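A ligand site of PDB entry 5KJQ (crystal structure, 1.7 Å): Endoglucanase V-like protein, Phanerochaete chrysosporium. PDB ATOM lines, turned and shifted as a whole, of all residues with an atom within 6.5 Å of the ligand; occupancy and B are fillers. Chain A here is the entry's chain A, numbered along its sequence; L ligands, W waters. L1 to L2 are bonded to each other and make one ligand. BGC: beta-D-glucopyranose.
Water W6 lies within hydrogen-bond range of O4 of BGC L2 (2.7 Å) and OD1 of Asn 92 (3.0 Å).
Water W5 lies within hydrogen-bond range of an oxygen (O3) of BGC L1 (2.7 Å) and the side-chain carboxylate of Glu 94 (2.8 Å).
Water W4 lies within hydrogen-bond range of an oxygen (O6) of BGC L2 (2.8 Å), the backbone NH (N) of Phe 95 (2.9 Å), the backbone carbonyl oxygen (O) of Asn 92 (3.4 Å) and the backbone NH (N) of Glu 94 (3.4 Å).
Water W7 bridges O3 of BGC L2 (2.9 Å) and N of Ser 19 (2.9 Å).
Water W1 lies within hydrogen-bond range of the side-chain carboxylate of Asp 114 (2.6 Å), an oxygen (O4) of BGC L2 (3.4 Å) and the side-chain sulfur of Cys 87 (3.7 Å).
The side-chain sulfur (SG) of Cys 87 is disulfide-bonded to the side-chain sulfur (SG) of Cys 96, 2.0 Å away.
The side-chain hydroxyl (OG1) of Thr 16 is in hydrogen-bond range of a ring nitrogen (NE2) of His 112 (2.8 Å).
The side-chain carboxylate of Asp 114 lies close to the backbone NH of Met 17 (3.4 Å).
ND2 of Asn 92 lies within hydrogen-bond range of O of Pro 88.
The side-chain carboxylate (OD1) of Asp 114 sits at hydrogen-bond distance from the side-chain hydroxyl (OG1) of Thr 16 (2.7 Å).
The side-chain hydroxyl (OH) of Tyr 67 lies within hydrogen-bond range of the side-chain carboxylate (OE2) of Glu 94, 2.4 Å away.
Merely in contact with the ligand: Thr 16 (3.2 Å), Tyr 18 (3.5 Å) and Phe 95 (3.3 Å).
Hydrophobic or aromatic side chains within 4 Å of the ligand: Met 17, Tyr 18, Tyr 67 and Phe 95.
Of the 20 residues printed, 8 come within 4 Å of the ligand.
The nearest printed residue that does not touch the ligand is Ala 132 (4.02 Å).
O4 of BGC L2 lies within hydrogen-bond range of OD2 of Asp 114 (2.5 Å).
O of Gly 131 sits at hydrogen-bond distance from O6 of BGC L1 (2.7 Å).
The side-chain hydroxyl of Tyr 67 is in hydrogen-bond range of an oxygen (O2) of BGC L1.
The backbone NH (N) of Met 17 is in hydrogen-bond range of an oxygen (O6) of BGC L1 (2.9 Å).
OD1 of Asn 92 is in hydrogen-bond range of O6 of BGC L2, 2.7 Å away.
The backbone carbonyl oxygen (O) of Met 17 is in hydrogen-bond range of an oxygen (O2) of BGC L2 (2.7 Å).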
ATOM      1  N   PHE A  15       9.599  -7.585 -28.656  1.00  0.00           N
ATOM      2  CA  PHE A  15       9.462  -8.986 -28.312  1.00  0.00           C
ATOM      3  C   PHE A  15      10.194  -9.270 -27.014  1.00  0.00           C
ATOM      4  O   PHE A  15      11.354  -8.877 -26.868  1.00  0.00           O
ATOM      5  CB  PHE A  15      10.048  -9.888 -29.409  1.00  0.00           C
ATOM      6  CG  PHE A  15       9.443  -9.648 -30.761  1.00  0.00           C
ATOM      7  CD1 PHE A  15       8.192 -10.169 -31.059  1.00  0.00           C
ATOM      8  CD2 PHE A  15      10.101  -8.877 -31.705  1.00  0.00           C
ATOM      9  CE1 PHE A  15       7.611  -9.941 -32.296  1.00  0.00           C
ATOM     10  CE2 PHE A  15       9.526  -8.629 -32.955  1.00  0.00           C
ATOM     11  CZ  PHE A  15       8.273  -9.187 -33.255  1.00  0.00           C
ATOM     12  N   THR A  16       9.518  -9.952 -26.098  1.00  0.00           N
ATOM     13  CA  THR A  16      10.180 -10.558 -24.955  1.00  0.00           C
ATOM     14  C   THR A  16       9.728 -12.010 -24.822  1.00  0.00           C
ATOM     15  O   THR A  16       8.990 -12.526 -25.670  1.00  0.00           O
ATOM     16  CB  THR A  16       9.871  -9.827 -23.654  1.00  0.00           C
ATOM     17  OG1 THR A  16       8.441  -9.659 -23.531  1.00  0.00           O
ATOM     18  CG2 THR A  16      10.564  -8.441 -23.607  1.00  0.00           C
ATOM     19  N   MET A  17      10.134 -12.648 -23.747  1.00  0.00           N
ATOM     20  CA  MET A  17       9.750 -14.010 -23.431  1.00  0.00           C
ATOM     21  C   MET A  17       9.309 -14.063 -21.970  1.00  0.00           C
ATOM     22  O   MET A  17       9.774 -13.278 -21.141  1.00  0.00           O
ATOM     23  CB  MET A  17      10.944 -14.923 -23.766  1.00  0.00           C
ATOM     24  CG  MET A  17      12.135 -14.756 -22.813  1.00  0.00           C
ATOM     25  SD  MET A  17      13.379 -16.037 -23.023  1.00  0.00           S
ATOM     26  CE  MET A  17      14.089 -15.607 -24.595  1.00  0.00           C
ATOM     27  N   TYR A  18       8.348 -14.949 -21.679  1.00  0.00           N
ATOM     28  CA  TYR A  18       7.862 -15.095 -20.317  1.00  0.00           C
ATOM     29  C   TYR A  18       7.562 -16.560 -20.020  1.00  0.00           C
ATOM     30  O   TYR A  18       7.445 -17.404 -20.914  1.00  0.00           O
ATOM     31  CB  TYR A  18       6.597 -14.255 -20.043  1.00  0.00           C
ATOM     32  CG  TYR A  18       5.271 -14.762 -20.582  1.00  0.00           C
ATOM     33  CD1 TYR A  18       4.976 -14.695 -21.944  1.00  0.00           C
ATOM     34  CD2 TYR A  18       4.287 -15.240 -19.739  1.00  0.00           C
ATOM     35  CE1 TYR A  18       3.754 -15.118 -22.453  1.00  0.00           C
ATOM     36  CE2 TYR A  18       3.039 -15.668 -20.229  1.00  0.00           C
ATOM     37  CZ  TYR A  18       2.787 -15.615 -21.591  1.00  0.00           C
ATOM     38  OH  TYR A  18       1.567 -16.017 -22.096  1.00  0.00           O
ATOM     39  N   SER A  19       7.439 -16.844 -18.726  1.00  0.00           N
ATOM     40  CA  SER A  19       7.221 -18.189 -18.241  1.00  0.00           C
ATOM     41  C   SER A  19       5.834 -18.324 -17.645  1.00  0.00           C
ATOM     42  O   SER A  19       5.332 -17.400 -16.987  1.00  0.00           O
ATOM     43  CB  SER A  19       8.263 -18.564 -17.180  1.00  0.00           C
ATOM     44  OG  SER A  19       9.515 -18.802 -17.791  1.00  0.00           O
ATOM     45  N   TYR A  67      18.854  -3.451 -26.798  1.00  0.00           N
ATOM     46  CA  TYR A  67      19.802  -3.362 -25.688  1.00  0.00           C
ATOM     47  C   TYR A  67      21.238  -3.500 -26.150  1.00  0.00           C
ATOM     48  O   TYR A  67      22.153  -3.076 -25.438  1.00  0.00           O
ATOM     49  CB  TYR A  67      19.525  -4.471 -24.659  1.00  0.00           C
ATOM     50  CG  TYR A  67      18.214  -4.352 -23.937  1.00  0.00           C
ATOM     51  CD1 TYR A  67      17.713  -3.105 -23.565  1.00  0.00           C
ATOM     52  CD2 TYR A  67      17.475  -5.478 -23.625  1.00  0.00           C
ATOM     53  CE1 TYR A  67      16.495  -3.002 -22.903  1.00  0.00           C
ATOM     54  CE2 TYR A  67      16.269  -5.382 -22.959  1.00  0.00           C
ATOM     55  CZ  TYR A  67      15.779  -4.146 -22.613  1.00  0.00           C
ATOM     56  OH  TYR A  67      14.580  -4.072 -21.955  1.00  0.00           O
ATOM     57  N   CYS A  87      -0.552  -9.028 -22.230  1.00  0.00           N
ATOM     58  CA  CYS A  87       0.528  -8.312 -21.582  1.00  0.00           C
ATOM     59  C   CYS A  87      -0.054  -6.968 -21.129  1.00  0.00           C
ATOM     60  O   CYS A  87      -0.204  -6.058 -21.955  1.00  0.00           O
ATOM     61  CB  CYS A  87       1.693  -8.110 -22.552  1.00  0.00           C
ATOM     62  SG  CYS A  87       3.145  -7.380 -21.757  1.00  0.00           S
ATOM     63  N   PRO A  88      -0.432  -6.806 -19.864  1.00  0.00           N
ATOM     64  CA  PRO A  88      -1.170  -5.604 -19.457  1.00  0.00           C
ATOM     65  C   PRO A  88      -0.259  -4.385 -19.328  1.00  0.00           C
ATOM     66  O   PRO A  88       0.953  -4.497 -19.116  1.00  0.00           O
ATOM     67  CB  PRO A  88      -1.742  -5.991 -18.086  1.00  0.00           C
ATOM     68  CG  PRO A  88      -0.744  -6.933 -17.535  1.00  0.00           C
ATOM     69  CD  PRO A  88      -0.178  -7.713 -18.726  1.00  0.00           C
ATOM     70  N   GLY A  91       2.342  -2.780 -14.752  1.00  0.00           N
ATOM     71  CA  GLY A  91       3.496  -3.597 -14.475  1.00  0.00           C
ATOM     72  C   GLY A  91       4.370  -3.926 -15.665  1.00  0.00           C
ATOM     73  O   GLY A  91       5.366  -4.638 -15.500  1.00  0.00           O
ATOM     74  N   ASN A  92       4.017  -3.441 -16.855  1.00  0.00           N
ATOM     75  CA  ASN A  92       4.800  -3.702 -18.064  1.00  0.00           C
ATOM     76  C   ASN A  92       4.927  -2.405 -18.875  1.00  0.00           C
ATOM     77  O   ASN A  92       4.642  -2.364 -20.075  1.00  0.00           O
ATOM     78  CB  ASN A  92       4.178  -4.811 -18.913  1.00  0.00           C
ATOM     79  CG  ASN A  92       4.060  -6.123 -18.158  1.00  0.00           C
ATOM     80  OD1 ASN A  92       5.028  -6.905 -18.080  1.00  0.00           O
ATOM     81  ND2 ASN A  92       2.880  -6.402 -17.618  1.00  0.00           N
ATOM     82  N   GLN A  93       5.367  -1.333 -18.231  1.00  0.00           N
ATOM     83  CA  GLN A  93       5.377  -0.048 -18.930  1.00  0.00           C
ATOM     84  C   GLN A  93       6.382  -0.043 -20.083  1.00  0.00           C
ATOM     85  O   GLN A  93       6.088   0.494 -21.159  1.00  0.00           O
ATOM     86  CB  GLN A  93       5.681   1.100 -17.964  1.00  0.00           C
ATOM     87  CG  GLN A  93       5.830   2.433 -18.673  1.00  0.00           C
ATOM     88  CD  GLN A  93       4.486   3.008 -19.091  1.00  0.00           C
ATOM     89  OE1 GLN A  93       3.428   2.533 -18.673  1.00  0.00           O
ATOM     90  NE2 GLN A  93       4.521   4.044 -19.934  1.00  0.00           N
ATOM     91  N   GLU A  94       7.574  -0.621 -19.880  1.00  0.00           N
ATOM     92  CA  GLU A  94       8.605  -0.578 -20.918  1.00  0.00           C
ATOM     93  C   GLU A  94       8.101  -1.160 -22.223  1.00  0.00           C
ATOM     94  O   GLU A  94       8.278  -0.558 -23.293  1.00  0.00           O
ATOM     95  CB  GLU A  94       9.863  -1.325 -20.447  1.00  0.00           C
ATOM     96  CG  GLU A  94      10.988  -1.325 -21.487  1.00  0.00           C
ATOM     97  CD  GLU A  94      12.258  -2.022 -21.021  1.00  0.00           C
ATOM     98  OE1 GLU A  94      12.309  -2.536 -19.880  1.00  0.00           O
ATOM     99  OE2 GLU A  94      13.222  -2.079 -21.809  1.00  0.00           O
ATOM    100  N   PHE A  95       7.452  -2.331 -22.165  1.00  0.00           N
ATOM    101  CA  PHE A  95       7.106  -3.056 -23.376  1.00  0.00           C
ATOM    102  C   PHE A  95       5.621  -3.055 -23.715  1.00  0.00           C
ATOM    103  O   PHE A  95       5.284  -3.084 -24.899  1.00  0.00           O
ATOM    104  CB  PHE A  95       7.608  -4.508 -23.287  1.00  0.00           C
ATOM    105  CG  PHE A  95       9.103  -4.623 -23.391  1.00  0.00           C
ATOM    106  CD1 PHE A  95       9.744  -4.383 -24.598  1.00  0.00           C
ATOM    107  CD2 PHE A  95       9.876  -4.941 -22.281  1.00  0.00           C
ATOM    108  CE1 PHE A  95      11.130  -4.470 -24.707  1.00  0.00           C
ATOM    109  CE2 PHE A  95      11.265  -5.034 -22.383  1.00  0.00           C
ATOM    110  CZ  PHE A  95      11.891  -4.796 -23.599  1.00  0.00           C
ATOM    111  N   CYS A  96       4.722  -2.999 -22.738  1.00  0.00           N
ATOM    112  CA  CYS A  96       3.297  -3.153 -23.010  1.00  0.00           C
ATOM    113  C   CYS A  96       2.487  -1.929 -22.600  1.00  0.00           C
ATOM    114  O   CYS A  96       1.259  -2.028 -22.444  1.00  0.00           O
ATOM    115  CB  CYS A  96       2.758  -4.414 -22.344  1.00  0.00           C
ATOM    116  SG  CYS A  96       3.612  -5.862 -23.017  1.00  0.00           S
ATOM    117  N   HIS A 112       3.479  -5.234 -28.945  1.00  0.00           N
ATOM    118  CA  HIS A 112       4.453  -6.062 -28.253  1.00  0.00           C
ATOM    119  C   HIS A 112       3.950  -7.487 -28.172  1.00  0.00           C
ATOM    120  O   HIS A 112       2.783  -7.711 -27.846  1.00  0.00           O
ATOM    121  CB  HIS A 112       4.740  -5.592 -26.827  1.00  0.00           C
ATOM    122  CG  HIS A 112       5.837  -6.367 -26.162  1.00  0.00           C
ATOM    123  ND1 HIS A 112       7.176  -6.107 -26.387  1.00  0.00           N
ATOM    124  CD2 HIS A 112       5.790  -7.424 -25.320  1.00  0.00           C
ATOM    125  CE1 HIS A 112       7.900  -6.964 -25.696  1.00  0.00           C
ATOM    126  NE2 HIS A 112       7.091  -7.776 -25.039  1.00  0.00           N
ATOM    127  N   ASP A 114       4.838 -10.942 -26.132  1.00  0.00           N
ATOM    128  CA  ASP A 114       5.543 -11.630 -25.057  1.00  0.00           C
ATOM    129  C   ASP A 114       5.411 -13.117 -25.358  1.00  0.00           C
ATOM    130  O   ASP A 114       4.329 -13.694 -25.201  1.00  0.00           O
ATOM    131  CB  ASP A 114       4.903 -11.237 -23.725  1.00  0.00           C
ATOM    132  CG  ASP A 114       5.827 -11.442 -22.525  1.00  0.00           C
ATOM    133  OD1 ASP A 114       7.020 -11.740 -22.709  1.00  0.00           O
ATOM    134  OD2 ASP A 114       5.323 -11.291 -21.383  1.00  0.00           O
ATOM    135  N   PHE A 126      14.631 -16.207 -29.928  1.00  0.00           N
ATOM    136  CA  PHE A 126      15.637 -15.386 -29.288  1.00  0.00           C
ATOM    137  C   PHE A 126      16.991 -16.075 -29.311  1.00  0.00           C
ATOM    138  O   PHE A 126      17.124 -17.161 -28.716  1.00  0.00           O
ATOM    139  CB  PHE A 126      15.249 -15.086 -27.853  1.00  0.00           C
ATOM    140  CG  PHE A 126      14.024 -14.223 -27.722  1.00  0.00           C
ATOM    141  CD1 PHE A 126      14.108 -12.856 -27.900  1.00  0.00           C
ATOM    142  CD2 PHE A 126      12.798 -14.793 -27.414  1.00  0.00           C
ATOM    143  CE1 PHE A 126      12.981 -12.053 -27.785  1.00  0.00           C
ATOM    144  CE2 PHE A 126      11.673 -14.000 -27.268  1.00  0.00           C
ATOM    145  CZ  PHE A 126      11.760 -12.621 -27.464  1.00  0.00           C
ATOM    146  N   HIS A 130      20.053 -12.814 -25.735  1.00  0.00           N
ATOM    147  CA  HIS A 130      19.318 -11.725 -26.354  1.00  0.00           C
ATOM    148  C   HIS A 130      17.833 -11.912 -26.018  1.00  0.00           C
ATOM    149  O   HIS A 130      17.070 -12.488 -26.786  1.00  0.00           O
ATOM    150  CB  HIS A 130      19.571 -11.670 -27.854  1.00  0.00           C
ATOM    151  CG  HIS A 130      21.014 -11.479 -28.211  1.00  0.00           C
ATOM    152  ND1 HIS A 130      21.566 -10.234 -28.441  1.00  0.00           N
ATOM    153  CD2 HIS A 130      22.016 -12.372 -28.355  1.00  0.00           C
ATOM    154  CE1 HIS A 130      22.850 -10.373 -28.716  1.00  0.00           C
ATOM    155  NE2 HIS A 130      23.148 -11.661 -28.675  1.00  0.00           N
ATOM    156  N   GLY A 131      17.439 -11.420 -24.841  1.00  0.00           N
ATOM    157  CA  GLY A 131      16.099 -11.629 -24.307  1.00  0.00           C
ATOM    158  C   GLY A 131      15.028 -10.678 -24.799  1.00  0.00           C
ATOM    159  O   GLY A 131      13.847 -10.947 -24.584  1.00  0.00           O
ATOM    160  N   ALA A 132      15.404  -9.578 -25.444  1.00  0.00           N
ATOM    161  CA  ALA A 132      14.433  -8.642 -25.983  1.00  0.00           C
ATOM    162  C   ALA A 132      14.870  -8.221 -27.372  1.00  0.00           C
ATOM    163  O   ALA A 132      16.059  -7.971 -27.619  1.00  0.00           O
ATOM    164  CB  ALA A 132      14.274  -7.425 -25.076  1.00  0.00           C
HETATM  165  C2  BGC L   1      13.676  -7.406 -20.553  1.00  0.00           C
HETATM  166  C3  BGC L   1      12.575  -7.964 -19.720  1.00  0.00           C
HETATM  167  C4  BGC L   1      12.092  -9.291 -20.248  1.00  0.00           C
HETATM  168  C5  BGC L   1      13.254 -10.255 -20.492  1.00  0.00           C
HETATM  169  C6  BGC L   1      12.809 -11.553 -21.117  1.00  0.00           C
HETATM  170  C1  BGC L   1      14.801  -8.423 -20.668  1.00  0.00           C
HETATM  171  O1  BGC L   1      15.830  -7.936 -21.400  1.00  0.00           O
HETATM  172  O2  BGC L   1      14.138  -6.170 -19.958  1.00  0.00           O
HETATM  173  O3  BGC L   1      11.480  -7.026 -19.707  1.00  0.00           O
HETATM  174  O4  BGC L   1      11.250  -9.850 -19.227  1.00  0.00           O
HETATM  175  O5  BGC L   1      14.283  -9.643 -21.350  1.00  0.00           O
HETATM  176  O6  BGC L   1      12.338 -11.363 -22.424  1.00  0.00           O
HETATM  177  C2  BGC L   2       9.274 -10.962 -18.611  1.00  0.00           C
HETATM  178  C3  BGC L   2       7.807 -11.086 -18.831  1.00  0.00           C
HETATM  179  C4  BGC L   2       7.141  -9.773 -19.041  1.00  0.00           C
HETATM  180  C5  BGC L   2       7.818  -9.034 -20.204  1.00  0.00           C
HETATM  181  C6  BGC L   2       7.146  -7.724 -20.481  1.00  0.00           C
HETATM  182  C1  BGC L   2       9.968 -10.114 -19.666  1.00  0.00           C
HETATM  183  O2  BGC L   2       9.845 -12.280 -18.585  1.00  0.00           O
HETATM  184  O3  BGC L   2       7.240 -11.783 -17.672  1.00  0.00           O
HETATM  185  O4  BGC L   2       5.746  -9.967 -19.342  1.00  0.00           O
HETATM  186  O5  BGC L   2       9.253  -8.821 -19.914  1.00  0.00           O
HETATM  187  O6  BGC L   2       7.374  -6.828 -19.424  1.00  0.00           O
HETATM  188  O   HOH W   1       2.868 -10.970 -20.746  1.00  0.00           O
HETATM  189  O   HOH W   2      11.882 -12.371 -17.048  1.00  0.00           O
HETATM  190  O   HOH W   3       9.542  -6.711 -17.431  1.00  0.00           O
HETATM  191  O   HOH W   4       7.553  -4.030 -19.787  1.00  0.00           O
HETATM  192  O   HOH W   5      11.118  -4.616 -18.458  1.00  0.00           O
HETATM  193  O   HOH W   6       3.350  -9.339 -18.358  1.00  0.00           O
HETATM  194  O   HOH W   7       7.978 -14.519 -17.078  1.00  0.00           O
HETATM  195  O   HOH W   8       7.509 -10.311 -15.497  1.00  0.00           O
